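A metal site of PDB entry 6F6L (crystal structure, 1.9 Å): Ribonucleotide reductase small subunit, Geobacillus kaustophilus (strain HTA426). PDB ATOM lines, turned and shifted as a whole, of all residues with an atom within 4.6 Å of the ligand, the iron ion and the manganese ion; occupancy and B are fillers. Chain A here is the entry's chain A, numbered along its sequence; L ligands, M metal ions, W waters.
The backbone carbonyl oxygen of Ser 187 lies within hydrogen-bond range of the side-chain hydroxyl of Thr 191.
O of Val 180 lies within hydrogen-bond range of N of Ala 185 (2.8 Å).
O of Val 256 is in hydrogen-bond range of OG1 of Thr 260 (3.0 Å).
Residues that only touch the ligand: Thr 191, Gly 78, Phe 79, Leu 184, Val 180, Phe 149, Gly 188, Leu 259, Val 86, Tyr 255, Val 256, Gly 82, Thr 260 and Ala 185.
Hydrophobic or aromatic side chains within 4 Å of the ligand: Phe 79, Val 86, Phe 149, Val 180, Ala 185, Tyr 255, Val 256 and Leu 259.
Of the 27 residues printed, 19 come within 4 Å of the ligand.
The nearest printed residue that does not touch the ligand is Leu 282 (4.01 Å).
Of the 27 residues printed, 4 come within 4 Å of the iron ion.
Of the 27 residues printed, 4 come within 4 Å of the manganese ion.
The side-chain carboxylate (OE2) of Glu 181 is bound to the iron ion.
Water W1 is bound to the iron ion.
The iron ion is bound by the side-chain carboxylate (OE2) of Glu 116, 2.1 Å away.
O2 of the ligand is bound to the iron ion (2.2 Å).
The iron ion is bound by the side-chain carboxylate (OE2) of Glu 216 (2.2 Å).
ND1 of His 219 is bound to the iron ion.
The iron ion has six donor atoms within binding distance.
The manganese ion is bound by O1 of the ligand, OE1 of Glu 116, OE1 of Glu 83, ND1 of His 119, water W1 and water W2.
The manganese ion has six donor atoms within binding distance.
Water W2 bridges OH of Tyr 189 (2.6 Å) and OE1 of Glu 216 (3.1 Å).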
ATOM      1  N   LEU A  75      12.102  14.045 -21.841  1.00  0.00           N
ATOM      2  CA  LEU A  75      13.305  14.413 -22.584  1.00  0.00           C
ATOM      3  C   LEU A  75      14.371  13.336 -22.483  1.00  0.00           C
ATOM      4  O   LEU A  75      15.006  12.995 -23.475  1.00  0.00           O
ATOM      5  CB  LEU A  75      13.849  15.737 -22.059  1.00  0.00           C
ATOM      6  CG  LEU A  75      14.296  16.737 -23.119  1.00  0.00           C
ATOM      7  CD1 LEU A  75      13.073  17.232 -23.903  1.00  0.00           C
ATOM      8  CD2 LEU A  75      15.029  17.908 -22.443  1.00  0.00           C
ATOM      9  N   GLY A  78      13.563  10.349 -24.601  1.00  0.00           N
ATOM     10  CA  GLY A  78      13.803  10.514 -26.023  1.00  0.00           C
ATOM     11  C   GLY A  78      15.265  10.383 -26.353  1.00  0.00           C
ATOM     12  O   GLY A  78      15.648   9.778 -27.363  1.00  0.00           O
ATOM     13  N   PHE A  79      16.115  10.979 -25.517  1.00  0.00           N
ATOM     14  CA  PHE A  79      17.551  10.862 -25.727  1.00  0.00           C
ATOM     15  C   PHE A  79      18.030   9.437 -25.536  1.00  0.00           C
ATOM     16  O   PHE A  79      18.863   8.970 -26.306  1.00  0.00           O
ATOM     17  CB  PHE A  79      18.315  11.771 -24.795  1.00  0.00           C
ATOM     18  CG  PHE A  79      18.626  13.108 -25.394  1.00  0.00           C
ATOM     19  CD1 PHE A  79      19.600  13.233 -26.368  1.00  0.00           C
ATOM     20  CD2 PHE A  79      17.908  14.228 -25.008  1.00  0.00           C
ATOM     21  CE1 PHE A  79      19.863  14.465 -26.923  1.00  0.00           C
ATOM     22  CE2 PHE A  79      18.189  15.491 -25.567  1.00  0.00           C
ATOM     23  CZ  PHE A  79      19.147  15.589 -26.520  1.00  0.00           C
ATOM     24  N   GLY A  82      17.177   7.428 -28.434  1.00  0.00           N
ATOM     25  CA  GLY A  82      17.874   8.004 -29.567  1.00  0.00           C
ATOM     26  C   GLY A  82      19.334   7.587 -29.648  1.00  0.00           C
ATOM     27  O   GLY A  82      19.811   7.169 -30.711  1.00  0.00           O
ATOM     28  N   GLU A  83      20.081   7.717 -28.532  1.00  0.00           N
ATOM     29  CA  GLU A  83      21.494   7.325 -28.513  1.00  0.00           C
ATOM     30  C   GLU A  83      21.638   5.847 -28.812  1.00  0.00           C
ATOM     31  O   GLU A  83      22.560   5.421 -29.530  1.00  0.00           O
ATOM     32  CB  GLU A  83      22.132   7.627 -27.141  1.00  0.00           C
ATOM     33  CG  GLU A  83      21.966   9.043 -26.608  1.00  0.00           C
ATOM     34  CD  GLU A  83      22.588  10.128 -27.481  1.00  0.00           C
ATOM     35  OE1 GLU A  83      23.372   9.789 -28.398  1.00  0.00           O
ATOM     36  OE2 GLU A  83      22.278  11.319 -27.234  1.00  0.00           O
ATOM     37  N   VAL A  86      20.963   5.188 -32.605  1.00  0.00           N
ATOM     38  CA  VAL A  86      22.038   5.597 -33.518  1.00  0.00           C
ATOM     39  C   VAL A  86      23.306   4.771 -33.282  1.00  0.00           C
ATOM     40  O   VAL A  86      24.084   4.558 -34.220  1.00  0.00           O
ATOM     41  CB  VAL A  86      22.337   7.118 -33.414  1.00  0.00           C
ATOM     42  CG1 VAL A  86      21.107   7.949 -33.853  1.00  0.00           C
ATOM     43  CG2 VAL A  86      22.801   7.497 -32.027  1.00  0.00           C
ATOM     44  N   PHE A 112      32.802   8.185 -34.416  1.00  0.00           N
ATOM     45  CA  PHE A 112      31.373   8.481 -34.372  1.00  0.00           C
ATOM     46  C   PHE A 112      30.640   7.410 -33.576  1.00  0.00           C
ATOM     47  O   PHE A 112      29.889   7.714 -32.634  1.00  0.00           O
ATOM     48  CB  PHE A 112      30.882   8.555 -35.832  1.00  0.00           C
ATOM     49  CG  PHE A 112      29.507   9.106 -36.034  1.00  0.00           C
ATOM     50  CD1 PHE A 112      29.203   9.719 -37.227  1.00  0.00           C
ATOM     51  CD2 PHE A 112      28.493   8.935 -35.122  1.00  0.00           C
ATOM     52  CE1 PHE A 112      27.971  10.233 -37.452  1.00  0.00           C
ATOM     53  CE2 PHE A 112      27.229   9.431 -35.369  1.00  0.00           C
ATOM     54  CZ  PHE A 112      26.953  10.065 -36.517  1.00  0.00           C
ATOM     55  N   GLU A 116      28.773   7.590 -29.771  1.00  0.00           N
ATOM     56  CA  GLU A 116      27.395   7.264 -29.470  1.00  0.00           C
ATOM     57  C   GLU A 116      27.321   6.234 -28.352  1.00  0.00           C
ATOM     58  O   GLU A 116      26.406   6.283 -27.495  1.00  0.00           O
ATOM     59  CB  GLU A 116      26.627   6.783 -30.710  1.00  0.00           C
ATOM     60  CG  GLU A 116      26.609   7.744 -31.890  1.00  0.00           C
ATOM     61  CD  GLU A 116      25.863   9.036 -31.636  1.00  0.00           C
ATOM     62  OE1 GLU A 116      25.377   9.295 -30.489  1.00  0.00           O
ATOM     63  OE2 GLU A 116      25.697   9.767 -32.628  1.00  0.00           O
ATOM     64  N   HIS A 119      27.457   8.091 -25.363  1.00  0.00           N
ATOM     65  CA  HIS A 119      26.226   8.821 -25.092  1.00  0.00           C
ATOM     66  C   HIS A 119      25.164   7.927 -24.451  1.00  0.00           C
ATOM     67  O   HIS A 119      24.437   8.373 -23.554  1.00  0.00           O
ATOM     68  CB  HIS A 119      25.676   9.410 -26.373  1.00  0.00           C
ATOM     69  CG  HIS A 119      26.620  10.378 -27.015  1.00  0.00           C
ATOM     70  ND1 HIS A 119      26.302  11.072 -28.162  1.00  0.00           N
ATOM     71  CD2 HIS A 119      27.864  10.767 -26.671  1.00  0.00           C
ATOM     72  CE1 HIS A 119      27.320  11.857 -28.489  1.00  0.00           C
ATOM     73  NE2 HIS A 119      28.299  11.669 -27.608  1.00  0.00           N
ATOM     74  N   PHE A 149      12.307   6.873 -34.846  1.00  0.00           N
ATOM     75  CA  PHE A 149      13.397   6.123 -34.215  1.00  0.00           C
ATOM     76  C   PHE A 149      13.200   4.613 -34.219  1.00  0.00           C
ATOM     77  O   PHE A 149      14.179   3.876 -34.299  1.00  0.00           O
ATOM     78  CB  PHE A 149      13.582   6.581 -32.771  1.00  0.00           C
ATOM     79  CG  PHE A 149      14.204   7.946 -32.655  1.00  0.00           C
ATOM     80  CD1 PHE A 149      15.568   8.107 -32.707  1.00  0.00           C
ATOM     81  CD2 PHE A 149      13.412   9.075 -32.521  1.00  0.00           C
ATOM     82  CE1 PHE A 149      16.156   9.344 -32.609  1.00  0.00           C
ATOM     83  CE2 PHE A 149      14.002  10.331 -32.445  1.00  0.00           C
ATOM     84  CZ  PHE A 149      15.376  10.447 -32.470  1.00  0.00           C
ATOM     85  N   VAL A 180      17.599  13.458 -37.087  1.00  0.00           N
ATOM     86  CA  VAL A 180      17.804  12.931 -35.732  1.00  0.00           C
ATOM     87  C   VAL A 180      18.820  13.773 -34.965  1.00  0.00           C
ATOM     88  O   VAL A 180      18.560  14.229 -33.839  1.00  0.00           O
ATOM     89  CB  VAL A 180      18.187  11.457 -35.800  1.00  0.00           C
ATOM     90  CG1 VAL A 180      18.753  10.941 -34.432  1.00  0.00           C
ATOM     91  CG2 VAL A 180      16.972  10.667 -36.242  1.00  0.00           C
ATOM     92  N   GLU A 181      20.003  13.973 -35.537  1.00  0.00           N
ATOM     93  CA  GLU A 181      21.080  14.689 -34.863  1.00  0.00           C
ATOM     94  C   GLU A 181      20.960  16.210 -35.039  1.00  0.00           C
ATOM     95  O   GLU A 181      20.917  16.951 -34.051  1.00  0.00           O
ATOM     96  CB  GLU A 181      22.435  14.205 -35.414  1.00  0.00           C
ATOM     97  CG  GLU A 181      22.805  12.817 -34.897  1.00  0.00           C
ATOM     98  CD  GLU A 181      24.087  12.289 -35.471  1.00  0.00           C
ATOM     99  OE1 GLU A 181      24.314  12.558 -36.673  1.00  0.00           O
ATOM    100  OE2 GLU A 181      24.863  11.632 -34.718  1.00  0.00           O
ATOM    101  N   LEU A 184      16.691  17.138 -34.063  1.00  0.00           N
ATOM    102  CA  LEU A 184      16.113  16.774 -32.770  1.00  0.00           C
ATOM    103  C   LEU A 184      17.149  16.821 -31.645  1.00  0.00           C
ATOM    104  O   LEU A 184      16.892  17.439 -30.608  1.00  0.00           O
ATOM    105  CB  LEU A 184      15.456  15.392 -32.854  1.00  0.00           C
ATOM    106  CG  LEU A 184      14.140  15.364 -33.614  1.00  0.00           C
ATOM    107  CD1 LEU A 184      13.802  13.906 -33.898  1.00  0.00           C
ATOM    108  CD2 LEU A 184      13.037  16.040 -32.822  1.00  0.00           C
ATOM    109  N   ALA A 185      18.335  16.230 -31.832  1.00  0.00           N
ATOM    110  CA  ALA A 185      19.317  16.223 -30.741  1.00  0.00           C
ATOM    111  C   ALA A 185      19.757  17.647 -30.381  1.00  0.00           C
ATOM    112  O   ALA A 185      19.866  17.995 -29.188  1.00  0.00           O
ATOM    113  CB  ALA A 185      20.542  15.391 -31.110  1.00  0.00           C
ATOM    114  N   SER A 187      18.102  20.443 -30.689  1.00  0.00           N
ATOM    115  CA  SER A 187      17.022  21.137 -30.011  1.00  0.00           C
ATOM    116  C   SER A 187      16.828  20.594 -28.610  1.00  0.00           C
ATOM    117  O   SER A 187      16.482  21.365 -27.712  1.00  0.00           O
ATOM    118  CB  SER A 187      15.732  21.020 -30.835  1.00  0.00           C
ATOM    119  OG  SER A 187      15.937  21.538 -32.146  1.00  0.00           O
ATOM    120  N   GLY A 188      17.083  19.296 -28.398  1.00  0.00           N
ATOM    121  CA  GLY A 188      17.111  18.737 -27.053  1.00  0.00           C
ATOM    122  C   GLY A 188      18.217  19.305 -26.171  1.00  0.00           C
ATOM    123  O   GLY A 188      17.997  19.543 -24.968  1.00  0.00           O
ATOM    124  N   TYR A 189      19.427  19.468 -26.711  1.00  0.00           N
ATOM    125  CA  TYR A 189      20.498  20.092 -25.936  1.00  0.00           C
ATOM    126  C   TYR A 189      20.073  21.492 -25.503  1.00  0.00           C
ATOM    127  O   TYR A 189      20.278  21.882 -24.348  1.00  0.00           O
ATOM    128  CB  TYR A 189      21.792  20.220 -26.739  1.00  0.00           C
ATOM    129  CG  TYR A 189      22.334  18.926 -27.248  1.00  0.00           C
ATOM    130  CD1 TYR A 189      22.202  17.781 -26.519  1.00  0.00           C
ATOM    131  CD2 TYR A 189      22.946  18.844 -28.489  1.00  0.00           C
ATOM    132  CE1 TYR A 189      22.678  16.566 -27.005  1.00  0.00           C
ATOM    133  CE2 TYR A 189      23.402  17.643 -28.977  1.00  0.00           C
ATOM    134  CZ  TYR A 189      23.274  16.511 -28.228  1.00  0.00           C
ATOM    135  OH  TYR A 189      23.721  15.286 -28.702  1.00  0.00           O
ATOM    136  N   THR A 191      17.024  22.675 -25.206  1.00  0.00           N
ATOM    137  CA  THR A 191      15.944  22.563 -24.249  1.00  0.00           C
ATOM    138  C   THR A 191      16.470  22.257 -22.847  1.00  0.00           C
ATOM    139  O   THR A 191      16.012  22.849 -21.855  1.00  0.00           O
ATOM    140  CB  THR A 191      14.947  21.496 -24.708  1.00  0.00           C
ATOM    141  OG1 THR A 191      14.369  21.874 -25.962  1.00  0.00           O
ATOM    142  CG2 THR A 191      13.826  21.270 -23.687  1.00  0.00           C
ATOM    143  N   GLU A 216      28.465  16.018 -31.133  1.00  0.00           N
ATOM    144  CA  GLU A 216      27.435  16.124 -32.179  1.00  0.00           C
ATOM    145  C   GLU A 216      27.895  16.967 -33.343  1.00  0.00           C
ATOM    146  O   GLU A 216      27.484  16.735 -34.481  1.00  0.00           O
ATOM    147  CB  GLU A 216      26.175  16.762 -31.617  1.00  0.00           C
ATOM    148  CG  GLU A 216      24.890  16.339 -32.261  1.00  0.00           C
ATOM    149  CD  GLU A 216      24.684  14.891 -31.991  1.00  0.00           C
ATOM    150  OE1 GLU A 216      24.193  14.583 -30.913  1.00  0.00           O
ATOM    151  OE2 GLU A 216      25.097  14.073 -32.849  1.00  0.00           O
ATOM    152  N   HIS A 219      29.425  14.837 -35.789  1.00  0.00           N
ATOM    153  CA  HIS A 219      28.455  13.930 -36.400  1.00  0.00           C
ATOM    154  C   HIS A 219      27.674  14.620 -37.503  1.00  0.00           C
ATOM    155  O   HIS A 219      27.477  14.052 -38.589  1.00  0.00           O
ATOM    156  CB  HIS A 219      27.499  13.377 -35.330  1.00  0.00           C
ATOM    157  CG  HIS A 219      28.202  12.645 -34.226  1.00  0.00           C
ATOM    158  ND1 HIS A 219      27.556  12.018 -33.182  1.00  0.00           N
ATOM    159  CD2 HIS A 219      29.524  12.470 -33.996  1.00  0.00           C
ATOM    160  CE1 HIS A 219      28.451  11.508 -32.353  1.00  0.00           C
ATOM    161  NE2 HIS A 219      29.655  11.758 -32.838  1.00  0.00           N
ATOM    162  N   TYR A 255       6.392  15.049 -32.624  1.00  0.00           N
ATOM    163  CA  TYR A 255       7.031  14.695 -31.347  1.00  0.00           C
ATOM    164  C   TYR A 255       7.193  15.938 -30.492  1.00  0.00           C
ATOM    165  O   TYR A 255       6.822  15.925 -29.305  1.00  0.00           O
ATOM    166  CB  TYR A 255       8.378  14.018 -31.608  1.00  0.00           C
ATOM    167  CG  TYR A 255       9.161  13.687 -30.370  1.00  0.00           C
ATOM    168  CD1 TYR A 255       8.618  12.899 -29.373  1.00  0.00           C
ATOM    169  CD2 TYR A 255      10.449  14.123 -30.228  1.00  0.00           C
ATOM    170  CE1 TYR A 255       9.336  12.569 -28.254  1.00  0.00           C
ATOM    171  CE2 TYR A 255      11.194  13.820 -29.077  1.00  0.00           C
ATOM    172  CZ  TYR A 255      10.621  13.036 -28.108  1.00  0.00           C
ATOM    173  OH  TYR A 255      11.348  12.712 -26.980  1.00  0.00           O
ATOM    174  N   VAL A 256       7.643  17.046 -31.089  1.00  0.00           N
ATOM    175  CA  VAL A 256       7.909  18.265 -30.334  1.00  0.00           C
ATOM    176  C   VAL A 256       6.625  18.805 -29.704  1.00  0.00           C
ATOM    177  O   VAL A 256       6.608  19.185 -28.541  1.00  0.00           O
ATOM    178  CB  VAL A 256       8.584  19.298 -31.265  1.00  0.00           C
ATOM    179  CG1 VAL A 256       8.493  20.673 -30.711  1.00  0.00           C
ATOM    180  CG2 VAL A 256      10.047  18.923 -31.489  1.00  0.00           C
ATOM    181  N   LEU A 259       5.870  16.616 -26.645  1.00  0.00           N
ATOM    182  CA  LEU A 259       6.653  17.038 -25.487  1.00  0.00           C
ATOM    183  C   LEU A 259       6.161  18.362 -24.938  1.00  0.00           C
ATOM    184  O   LEU A 259       6.144  18.559 -23.716  1.00  0.00           O
ATOM    185  CB  LEU A 259       8.122  17.178 -25.851  1.00  0.00           C
ATOM    186  CG  LEU A 259       8.856  15.877 -26.162  1.00  0.00           C
ATOM    187  CD1 LEU A 259      10.270  16.228 -26.605  1.00  0.00           C
ATOM    188  CD2 LEU A 259       8.868  14.965 -24.963  1.00  0.00           C
ATOM    189  N   THR A 260       5.816  19.303 -25.834  1.00  0.00           N
ATOM    190  CA  THR A 260       5.379  20.624 -25.415  1.00  0.00           C
ATOM    191  C   THR A 260       4.089  20.534 -24.627  1.00  0.00           C
ATOM    192  O   THR A 260       3.901  21.252 -23.630  1.00  0.00           O
ATOM    193  CB  THR A 260       5.176  21.510 -26.635  1.00  0.00           C
ATOM    194  OG1 THR A 260       6.447  21.826 -27.210  1.00  0.00           O
ATOM    195  CG2 THR A 260       4.515  22.787 -26.260  1.00  0.00           C
ATOM    196  N   TYR A 279       7.723  27.718 -24.110  1.00  0.00           N
ATOM    197  CA  TYR A 279       7.593  26.574 -25.012  1.00  0.00           C
ATOM    198  C   TYR A 279       7.470  27.015 -26.462  1.00  0.00           C
ATOM    199  O   TYR A 279       7.770  26.231 -27.364  1.00  0.00           O
ATOM    200  CB  TYR A 279       6.397  25.715 -24.635  1.00  0.00           C
ATOM    201  CG  TYR A 279       6.685  24.885 -23.433  1.00  0.00           C
ATOM    202  CD1 TYR A 279       7.561  23.815 -23.500  1.00  0.00           C
ATOM    203  CD2 TYR A 279       6.120  25.199 -22.196  1.00  0.00           C
ATOM    204  CE1 TYR A 279       7.863  23.068 -22.381  1.00  0.00           C
ATOM    205  CE2 TYR A 279       6.408  24.454 -21.075  1.00  0.00           C
ATOM    206  CZ  TYR A 279       7.276  23.392 -21.162  1.00  0.00           C
ATOM    207  OH  TYR A 279       7.571  22.649 -20.048  1.00  0.00           O
ATOM    208  N   LEU A 282      11.009  27.390 -27.685  1.00  0.00           N
ATOM    209  CA  LEU A 282      11.571  26.069 -27.955  1.00  0.00           C
ATOM    210  C   LEU A 282      11.113  25.558 -29.309  1.00  0.00           C
ATOM    211  O   LEU A 282      11.942  25.133 -30.131  1.00  0.00           O
ATOM    212  CB  LEU A 282      11.194  25.085 -26.852  1.00  0.00           C
ATOM    213  CG  LEU A 282      11.768  25.494 -25.478  1.00  0.00           C
ATOM    214  CD1 LEU A 282      11.292  24.594 -24.327  1.00  0.00           C
ATOM    215  CD2 LEU A 282      13.299  25.547 -25.490  1.00  0.00           C
ATOM    216  N   VAL A 286      13.343  24.472 -32.871  1.00  0.00           N
ATOM    217  CA  VAL A 286      13.238  23.267 -33.706  1.00  0.00           C
ATOM    218  C   VAL A 286      13.077  23.656 -35.173  1.00  0.00           C
ATOM    219  O   VAL A 286      13.748  23.108 -36.061  1.00  0.00           O
ATOM    220  CB  VAL A 286      12.074  22.387 -33.231  1.00  0.00           C
ATOM    221  CG1 VAL A 286      11.829  21.220 -34.192  1.00  0.00           C
ATOM    222  CG2 VAL A 286      12.375  21.868 -31.852  1.00  0.00           C
HETATM  223  C1  LIG L   1      22.627  11.264 -31.512  1.00  0.00           C
HETATM  224  O1  LIG L   1      23.169  11.212 -30.392  1.00  0.00           O
HETATM  225  O2  LIG L   1      23.202  11.252 -32.605  1.00  0.00           O
HETATM  226  C2  LIG L   1      21.058  11.394 -31.596  1.00  0.00           C
HETATM  227  C3  LIG L   1      20.237  11.496 -30.314  1.00  0.00           C
HETATM  228  C4  LIG L   1      18.707  11.744 -30.589  1.00  0.00           C
HETATM  229  C5  LIG L   1      17.933  12.450 -29.443  1.00  0.00           C
HETATM  230  C6  LIG L   1      16.428  12.601 -29.672  1.00  0.00           C
HETATM  231  C7  LIG L   1      15.609  13.146 -28.450  1.00  0.00           C
HETATM  232  C8  LIG L   1      15.733  14.629 -28.312  1.00  0.00           C
HETATM  233  C9  LIG L   1      14.538  15.359 -27.709  1.00  0.00           C
HETATM  234  C10 LIG L   1      13.975  16.448 -28.644  1.00  0.00           C
HETATM  235  C11 LIG L   1      13.685  17.723 -27.966  1.00  0.00           C
HETATM  236  C12 LIG L   1      12.828  18.649 -28.798  1.00  0.00           C
HETATM  237  C13 LIG L   1      12.397  19.886 -28.011  1.00  0.00           C
HETATM  238  C14 LIG L   1      10.991  19.841 -27.438  1.00  0.00           C
HETATM  239  C15 LIG L   1      10.594  21.120 -26.666  1.00  0.00           C
HETATM  240  C16 LIG L   1       9.829  20.880 -25.331  1.00  0.00           C
HETATM  241 FE    FE M   1      25.329  11.856 -32.769  1.00  0.00          FE
HETATM  242 MN    MN M   2      24.657  10.991 -29.532  1.00  0.00          MN
HETATM  243  O   HOH W   1      25.735  12.410 -30.808  1.00  0.00           O
HETATM  244  O   HOH W   2      23.540  12.716 -28.476  1.00  0.00           O
